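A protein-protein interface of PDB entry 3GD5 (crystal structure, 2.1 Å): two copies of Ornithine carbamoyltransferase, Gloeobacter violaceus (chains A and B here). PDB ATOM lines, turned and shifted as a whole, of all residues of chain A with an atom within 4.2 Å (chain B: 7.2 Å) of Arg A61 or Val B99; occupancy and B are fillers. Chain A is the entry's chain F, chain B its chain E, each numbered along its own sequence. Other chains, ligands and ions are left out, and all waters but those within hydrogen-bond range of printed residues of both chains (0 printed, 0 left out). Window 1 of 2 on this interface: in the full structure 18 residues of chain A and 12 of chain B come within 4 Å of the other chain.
Hydrophobic or aromatic side chains of chain A that line the printed part of chain B: Val A64 and Pro A274.
The side-chain hydroxyl (OH) of Tyr B103 lies within hydrogen-bond range of the backbone carbonyl oxygen (O) of Ala A297 (2.4 Å).
NH2 of Arg A61 is in salt-bridge range of OE2 of Glu B91 (3.0 Å).
Of the printed residues of chain A, Glu B91 touches Arg A61 and Pro A274.
Printed residues of chain A within 4 Å of Tyr B103: Val A64, Ser A65 and Ala A297.
Of the printed residues of chain A, Leu B80 touches Thr A60 and Arg A63.
Of the printed residues of chain B, Val A64 touches Tyr B103.
Of the printed residues of chain B, Ala A297 touches Tyr B103 (2.4 Å).
Val B104 touches none of the printed residues of chain A.
Tyr B123 touches none of the printed residues of chain A.
The nearest residue of chain B that does not touch Arg A61 is Tyr B103 (4.1 Å).
OG of Ser A65 sits at hydrogen-bond distance from O of Thr A62 (3.2 Å).
The backbone carbonyl oxygen (O) of Arg A61 is in hydrogen-bond range of the side-chain hydroxyl (OG) of Ser A65 (3.0 Å).
Among the printed residues, merely in contact across the chains: Thr A60 with Leu B80 (3.6 Å), Arg A61 with Val B99 (3.8 Å), Arg A63 with Leu B80 (3.7 Å), Val A64 with Tyr B103 (3.6 Å), Ser A65 with Tyr B103 (3.8 Å) and Pro A274 with Glu B91 (3.7 Å).
No position is printed for both chains.
Of the 8 pairs that touch across the chains among the printed residues, none has its exchanged pair printed and touching as well.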
ATOM      1  N   SER A  59     -28.880 -16.120  10.322  1.00  0.00           N
ATOM      2  CA  SER A  59     -27.853 -15.373  11.040  1.00  0.00           C
ATOM      3  C   SER A  59     -26.502 -15.824  10.490  1.00  0.00           C
ATOM      4  O   SER A  59     -25.863 -16.723  11.038  1.00  0.00           O
ATOM      5  CB  SER A  59     -27.951 -15.663  12.546  1.00  0.00           C
ATOM      6  OG  SER A  59     -27.103 -14.811  13.307  1.00  0.00           O
ATOM      7  N   THR A  60     -26.081 -15.200   9.394  1.00  0.00           N
ATOM      8  CA  THR A  60     -24.822 -15.538   8.736  1.00  0.00           C
ATOM      9  C   THR A  60     -23.611 -15.438   9.660  1.00  0.00           C
ATOM     10  O   THR A  60     -22.809 -16.366   9.742  1.00  0.00           O
ATOM     11  CB  THR A  60     -24.604 -14.643   7.487  1.00  0.00           C
ATOM     12  OG1 THR A  60     -25.621 -14.930   6.515  1.00  0.00           O
ATOM     13  CG2 THR A  60     -23.232 -14.896   6.867  1.00  0.00           C
ATOM     14  N   ARG A  61     -23.478 -14.310  10.344  1.00  0.00           N
ATOM     15  CA  ARG A  61     -22.379 -14.090  11.279  1.00  0.00           C
ATOM     16  C   ARG A  61     -22.304 -15.267  12.251  1.00  0.00           C
ATOM     17  O   ARG A  61     -21.221 -15.784  12.560  1.00  0.00           O
ATOM     18  CB  ARG A  61     -22.644 -12.803  12.051  1.00  0.00           C
ATOM     19  CG  ARG A  61     -21.662 -12.470  13.154  1.00  0.00           C
ATOM     20  CD  ARG A  61     -22.285 -11.423  14.079  1.00  0.00           C
ATOM     21  NE  ARG A  61     -23.073 -10.440  13.335  1.00  0.00           N
ATOM     22  CZ  ARG A  61     -22.566  -9.589  12.450  1.00  0.00           C
ATOM     23  NH1 ARG A  61     -21.262  -9.595  12.202  1.00  0.00           N
ATOM     24  NH2 ARG A  61     -23.357  -8.742  11.801  1.00  0.00           N
ATOM     25  N   THR A  62     -23.476 -15.689  12.723  1.00  0.00           N
ATOM     26  CA  THR A  62     -23.573 -16.793  13.662  1.00  0.00           C
ATOM     27  C   THR A  62     -23.291 -18.134  12.998  1.00  0.00           C
ATOM     28  O   THR A  62     -22.630 -18.992  13.581  1.00  0.00           O
ATOM     29  CB  THR A  62     -24.969 -16.850  14.318  1.00  0.00           C
ATOM     30  OG1 THR A  62     -25.245 -15.607  14.975  1.00  0.00           O
ATOM     31  CG2 THR A  62     -25.020 -17.974  15.354  1.00  0.00           C
ATOM     32  N   ARG A  63     -23.787 -18.321  11.782  1.00  0.00           N
ATOM     33  CA  ARG A  63     -23.564 -19.582  11.089  1.00  0.00           C
ATOM     34  C   ARG A  63     -22.092 -19.760  10.712  1.00  0.00           C
ATOM     35  O   ARG A  63     -21.530 -20.845  10.887  1.00  0.00           O
ATOM     36  CB  ARG A  63     -24.452 -19.678   9.845  1.00  0.00           C
ATOM     37  CG  ARG A  63     -24.547 -21.089   9.281  1.00  0.00           C
ATOM     38  CD  ARG A  63     -25.853 -21.292   8.512  1.00  0.00           C
ATOM     39  NE  ARG A  63     -26.006 -20.298   7.457  1.00  0.00           N
ATOM     40  CZ  ARG A  63     -25.197 -20.207   6.410  1.00  0.00           C
ATOM     41  NH1 ARG A  63     -24.185 -21.057   6.284  1.00  0.00           N
ATOM     42  NH2 ARG A  63     -25.391 -19.261   5.498  1.00  0.00           N
ATOM     43  N   VAL A  64     -21.465 -18.698  10.214  1.00  0.00           N
ATOM     44  CA  VAL A  64     -20.057 -18.785   9.842  1.00  0.00           C
ATOM     45  C   VAL A  64     -19.147 -19.012  11.059  1.00  0.00           C
ATOM     46  O   VAL A  64     -18.272 -19.877  11.019  1.00  0.00           O
ATOM     47  CB  VAL A  64     -19.588 -17.520   9.072  1.00  0.00           C
ATOM     48  CG1 VAL A  64     -19.966 -16.278   9.843  1.00  0.00           C
ATOM     49  CG2 VAL A  64     -18.070 -17.575   8.851  1.00  0.00           C
ATOM     50  N   SER A  65     -19.352 -18.267  12.145  1.00  0.00           N
ATOM     51  CA  SER A  65     -18.499 -18.454  13.316  1.00  0.00           C
ATOM     52  C   SER A  65     -18.621 -19.854  13.920  1.00  0.00           C
ATOM     53  O   SER A  65     -17.628 -20.416  14.378  1.00  0.00           O
ATOM     54  CB  SER A  65     -18.770 -17.377  14.384  1.00  0.00           C
ATOM     55  OG  SER A  65     -20.121 -17.373  14.823  1.00  0.00           O
ATOM     56  N   LEU A 273     -22.717  -6.282  17.143  1.00  0.00           N
ATOM     57  CA  LEU A 273     -23.060  -6.203  15.721  1.00  0.00           C
ATOM     58  C   LEU A 273     -24.388  -6.890  15.469  1.00  0.00           C
ATOM     59  O   LEU A 273     -24.809  -7.728  16.256  1.00  0.00           O
ATOM     60  CB  LEU A 273     -21.965  -6.860  14.864  1.00  0.00           C
ATOM     61  CG  LEU A 273     -20.594  -6.167  14.907  1.00  0.00           C
ATOM     62  CD1 LEU A 273     -19.583  -6.924  14.053  1.00  0.00           C
ATOM     63  CD2 LEU A 273     -20.748  -4.740  14.393  1.00  0.00           C
ATOM     64  N   PRO A 274     -25.087  -6.519  14.385  1.00  0.00           N
ATOM     65  CA  PRO A 274     -24.665  -5.494  13.424  1.00  0.00           C
ATOM     66  C   PRO A 274     -24.900  -4.131  14.069  1.00  0.00           C
ATOM     67  O   PRO A 274     -25.611  -4.033  15.067  1.00  0.00           O
ATOM     68  CB  PRO A 274     -25.586  -5.746  12.240  1.00  0.00           C
ATOM     69  CG  PRO A 274     -26.883  -6.106  12.938  1.00  0.00           C
ATOM     70  CD  PRO A 274     -26.406  -7.071  14.024  1.00  0.00           C
ATOM     71  N   ALA A 297     -15.591  -9.593  17.382  1.00  0.00           N
ATOM     72  CA  ALA A 297     -16.284 -10.407  16.383  1.00  0.00           C
ATOM     73  C   ALA A 297     -15.513 -11.690  16.074  1.00  0.00           C
ATOM     74  O   ALA A 297     -16.103 -12.768  15.922  1.00  0.00           O
ATOM     75  CB  ALA A 297     -16.488  -9.602  15.109  1.00  0.00           C
ATOM     76  N   LEU B  80     -22.660 -18.581   1.788  1.00  0.00           N
ATOM     77  CA  LEU B  80     -23.205 -17.381   2.422  1.00  0.00           C
ATOM     78  C   LEU B  80     -24.056 -16.576   1.444  1.00  0.00           C
ATOM     79  O   LEU B  80     -24.806 -17.139   0.646  1.00  0.00           O
ATOM     80  CB  LEU B  80     -22.083 -16.485   2.963  1.00  0.00           C
ATOM     81  CG  LEU B  80     -21.174 -16.989   4.089  1.00  0.00           C
ATOM     82  CD1 LEU B  80     -21.995 -17.814   5.069  1.00  0.00           C
ATOM     83  CD2 LEU B  80     -20.051 -17.826   3.524  1.00  0.00           C
ATOM     84  N   GLU B  91     -26.855  -4.406   6.348  1.00  0.00           N
ATOM     85  CA  GLU B  91     -25.553  -4.126   6.949  1.00  0.00           C
ATOM     86  C   GLU B  91     -24.584  -3.641   5.878  1.00  0.00           C
ATOM     87  O   GLU B  91     -24.600  -4.135   4.755  1.00  0.00           O
ATOM     88  CB  GLU B  91     -24.992  -5.390   7.616  1.00  0.00           C
ATOM     89  CG  GLU B  91     -23.586  -5.230   8.183  1.00  0.00           C
ATOM     90  CD  GLU B  91     -23.069  -6.484   8.882  1.00  0.00           C
ATOM     91  OE1 GLU B  91     -23.080  -7.566   8.256  1.00  0.00           O
ATOM     92  OE2 GLU B  91     -22.643  -6.385  10.054  1.00  0.00           O
ATOM     93  N   VAL B  93     -21.451  -3.425   3.602  1.00  0.00           N
ATOM     94  CA  VAL B  93     -20.469  -4.413   3.161  1.00  0.00           C
ATOM     95  C   VAL B  93     -19.110  -4.309   3.836  1.00  0.00           C
ATOM     96  O   VAL B  93     -18.446  -5.319   4.030  1.00  0.00           O
ATOM     97  CB  VAL B  93     -20.229  -4.349   1.627  1.00  0.00           C
ATOM     98  CG1 VAL B  93     -21.515  -4.634   0.882  1.00  0.00           C
ATOM     99  CG2 VAL B  93     -19.679  -2.998   1.243  1.00  0.00           C
ATOM    100  N   ARG B  94     -18.684  -3.101   4.187  1.00  0.00           N
ATOM    101  CA  ARG B  94     -17.385  -2.952   4.832  1.00  0.00           C
ATOM    102  C   ARG B  94     -17.399  -3.619   6.203  1.00  0.00           C
ATOM    103  O   ARG B  94     -16.354  -4.033   6.708  1.00  0.00           O
ATOM    104  CB  ARG B  94     -16.995  -1.471   4.950  1.00  0.00           C
ATOM    105  CG  ARG B  94     -18.012  -0.559   5.642  1.00  0.00           C
ATOM    106  CD  ARG B  94     -17.546   0.894   5.560  1.00  0.00           C
ATOM    107  NE  ARG B  94     -18.388   1.830   6.308  1.00  0.00           N
ATOM    108  CZ  ARG B  94     -19.628   2.174   5.970  1.00  0.00           C
ATOM    109  NH1 ARG B  94     -20.197   1.661   4.884  1.00  0.00           N
ATOM    110  NH2 ARG B  94     -20.302   3.038   6.721  1.00  0.00           N
ATOM    111  N   ASP B  95     -18.587  -3.731   6.795  1.00  0.00           N
ATOM    112  CA  ASP B  95     -18.740  -4.366   8.100  1.00  0.00           C
ATOM    113  C   ASP B  95     -18.761  -5.878   7.970  1.00  0.00           C
ATOM    114  O   ASP B  95     -18.096  -6.590   8.723  1.00  0.00           O
ATOM    115  CB  ASP B  95     -20.038  -3.917   8.775  1.00  0.00           C
ATOM    116  CG  ASP B  95     -19.921  -2.550   9.404  1.00  0.00           C
ATOM    117  OD1 ASP B  95     -18.849  -1.931   9.269  1.00  0.00           O
ATOM    118  OD2 ASP B  95     -20.898  -2.098  10.029  1.00  0.00           O
ATOM    119  N   THR B  96     -19.533  -6.363   7.007  1.00  0.00           N
ATOM    120  CA  THR B  96     -19.645  -7.793   6.798  1.00  0.00           C
ATOM    121  C   THR B  96     -18.380  -8.384   6.188  1.00  0.00           C
ATOM    122  O   THR B  96     -18.076  -9.557   6.416  1.00  0.00           O
ATOM    123  CB  THR B  96     -20.898  -8.137   5.944  1.00  0.00           C
ATOM    124  OG1 THR B  96     -20.573  -9.151   4.985  1.00  0.00           O
ATOM    125  CG2 THR B  96     -21.427  -6.910   5.249  1.00  0.00           C
ATOM    126  N   ALA B  97     -17.629  -7.569   5.447  1.00  0.00           N
ATOM    127  CA  ALA B  97     -16.392  -8.026   4.816  1.00  0.00           C
ATOM    128  C   ALA B  97     -15.274  -8.187   5.842  1.00  0.00           C
ATOM    129  O   ALA B  97     -14.523  -9.169   5.816  1.00  0.00           O
ATOM    130  CB  ALA B  97     -15.962  -7.043   3.731  1.00  0.00           C
ATOM    131  N   ARG B  98     -15.157  -7.206   6.733  1.00  0.00           N
ATOM    132  CA  ARG B  98     -14.138  -7.234   7.769  1.00  0.00           C
ATOM    133  C   ARG B  98     -14.400  -8.347   8.781  1.00  0.00           C
ATOM    134  O   ARG B  98     -13.466  -8.954   9.290  1.00  0.00           O
ATOM    135  CB  ARG B  98     -14.071  -5.880   8.485  1.00  0.00           C
ATOM    136  CG  ARG B  98     -13.358  -4.802   7.685  1.00  0.00           C
ATOM    137  CD  ARG B  98     -13.352  -3.443   8.407  1.00  0.00           C
ATOM    138  NE  ARG B  98     -14.677  -2.828   8.448  1.00  0.00           N
ATOM    139  CZ  ARG B  98     -14.930  -1.614   8.927  1.00  0.00           C
ATOM    140  NH1 ARG B  98     -13.946  -0.867   9.415  1.00  0.00           N
ATOM    141  NH2 ARG B  98     -16.170  -1.140   8.909  1.00  0.00           N
ATOM    142  N   VAL B  99     -15.665  -8.611   9.091  1.00  0.00           N
ATOM    143  CA  VAL B  99     -15.961  -9.679  10.032  1.00  0.00           C
ATOM    144  C   VAL B  99     -15.653 -11.008   9.319  1.00  0.00           C
ATOM    145  O   VAL B  99     -14.953 -11.864   9.853  1.00  0.00           O
ATOM    146  CB  VAL B  99     -17.445  -9.605  10.546  1.00  0.00           C
ATOM    147  CG1 VAL B  99     -18.419  -9.608   9.386  1.00  0.00           C
ATOM    148  CG2 VAL B  99     -17.747 -10.774  11.457  1.00  0.00           C
ATOM    149  N   LEU B 100     -16.135 -11.155   8.090  1.00  0.00           N
ATOM    150  CA  LEU B 100     -15.892 -12.372   7.322  1.00  0.00           C
ATOM    151  C   LEU B 100     -14.387 -12.610   7.219  1.00  0.00           C
ATOM    152  O   LEU B 100     -13.911 -13.745   7.336  1.00  0.00           O
ATOM    153  CB  LEU B 100     -16.497 -12.220   5.929  1.00  0.00           C
ATOM    154  CG  LEU B 100     -17.687 -13.092   5.524  1.00  0.00           C
ATOM    155  CD1 LEU B 100     -18.518 -13.511   6.733  1.00  0.00           C
ATOM    156  CD2 LEU B 100     -18.524 -12.318   4.523  1.00  0.00           C
ATOM    157  N   GLY B 101     -13.642 -11.529   7.010  1.00  0.00           N
ATOM    158  CA  GLY B 101     -12.199 -11.634   6.898  1.00  0.00           C
ATOM    159  C   GLY B 101     -11.534 -12.151   8.162  1.00  0.00           C
ATOM    160  O   GLY B 101     -10.335 -12.447   8.165  1.00  0.00           O
ATOM    161  N   ARG B 102     -12.307 -12.250   9.242  1.00  0.00           N
ATOM    162  CA  ARG B 102     -11.779 -12.750  10.508  1.00  0.00           C
ATOM    163  C   ARG B 102     -12.100 -14.230  10.692  1.00  0.00           C
ATOM    164  O   ARG B 102     -11.539 -14.887  11.573  1.00  0.00           O
ATOM    165  CB  ARG B 102     -12.364 -11.971  11.695  1.00  0.00           C
ATOM    166  CG  ARG B 102     -11.940 -10.509  11.786  1.00  0.00           C
ATOM    167  CD  ARG B 102     -10.433 -10.364  11.833  1.00  0.00           C
ATOM    168  NE  ARG B 102     -10.041  -8.994  12.131  1.00  0.00           N
ATOM    169  CZ  ARG B 102      -9.769  -8.535  13.351  1.00  0.00           C
ATOM    170  NH1 ARG B 102      -9.832  -9.338  14.407  1.00  0.00           N
ATOM    171  NH2 ARG B 102      -9.461  -7.258  13.518  1.00  0.00           N
ATOM    172  N   TYR B 103     -12.998 -14.757   9.864  1.00  0.00           N
ATOM    173  CA  TYR B 103     -13.388 -16.156   9.991  1.00  0.00           C
ATOM    174  C   TYR B 103     -12.846 -17.090   8.916  1.00  0.00           C
ATOM    175  O   TYR B 103     -12.336 -18.166   9.227  1.00  0.00           O
ATOM    176  CB  TYR B 103     -14.913 -16.284  10.010  1.00  0.00           C
ATOM    177  CG  TYR B 103     -15.609 -15.535  11.124  1.00  0.00           C
ATOM    178  CD1 TYR B 103     -15.073 -15.495  12.416  1.00  0.00           C
ATOM    179  CD2 TYR B 103     -16.829 -14.897  10.890  1.00  0.00           C
ATOM    180  CE1 TYR B 103     -15.739 -14.830  13.452  1.00  0.00           C
ATOM    181  CE2 TYR B 103     -17.510 -14.232  11.916  1.00  0.00           C
ATOM    182  CZ  TYR B 103     -16.964 -14.200  13.191  1.00  0.00           C
ATOM    183  OH  TYR B 103     -17.646 -13.538  14.190  1.00  0.00           O
ATOM    184  N   VAL B 104     -12.978 -16.689   7.653  1.00  0.00           N
ATOM    185  CA  VAL B 104     -12.524 -17.516   6.542  1.00  0.00           C
ATOM    186  C   VAL B 104     -11.257 -16.970   5.903  1.00  0.00           C
ATOM    187  O   VAL B 104     -10.774 -15.903   6.276  1.00  0.00           O
ATOM    188  CB  VAL B 104     -13.626 -17.658   5.472  1.00  0.00           C
ATOM    189  CG1 VAL B 104     -14.871 -18.316   6.090  1.00  0.00           C
ATOM    190  CG2 VAL B 104     -13.968 -16.291   4.898  1.00  0.00           C
ATOM    191  N   TYR B 123     -12.131  -4.187   1.882  1.00  0.00           N
ATOM    192  CA  TYR B 123     -12.178  -4.350   3.338  1.00  0.00           C
ATOM    193  C   TYR B 123     -11.943  -5.748   3.908  1.00  0.00           C
ATOM    194  O   TYR B 123     -11.496  -5.885   5.048  1.00  0.00           O
ATOM    195  CB  TYR B 123     -13.532  -3.864   3.858  1.00  0.00           C
ATOM    196  CG  TYR B 123     -13.808  -2.393   3.660  1.00  0.00           C
ATOM    197  CD1 TYR B 123     -13.330  -1.445   4.567  1.00  0.00           C
ATOM    198  CD2 TYR B 123     -14.579  -1.949   2.587  1.00  0.00           C
ATOM    199  CE1 TYR B 123     -13.623  -0.088   4.413  1.00  0.00           C
ATOM    200  CE2 TYR B 123     -14.875  -0.595   2.423  1.00  0.00           C
ATOM    201  CZ  TYR B 123     -14.394   0.329   3.342  1.00  0.00           C
ATOM    202  OH  TYR B 123     -14.691   1.664   3.183  1.00  0.00           O
ATOM    203  N   ALA B 124     -12.257  -6.777   3.130  1.00  0.00           N
ATOM    204  CA  ALA B 124     -12.124  -8.155   3.585  1.00  0.00           C
ATOM    205  C   ALA B 124     -10.794  -8.533   4.235  1.00  0.00           C
ATOM    206  O   ALA B 124     -10.783  -9.220   5.265  1.00  0.00           O
ATOM    207  CB  ALA B 124     -12.433  -9.110   2.433  1.00  0.00           C
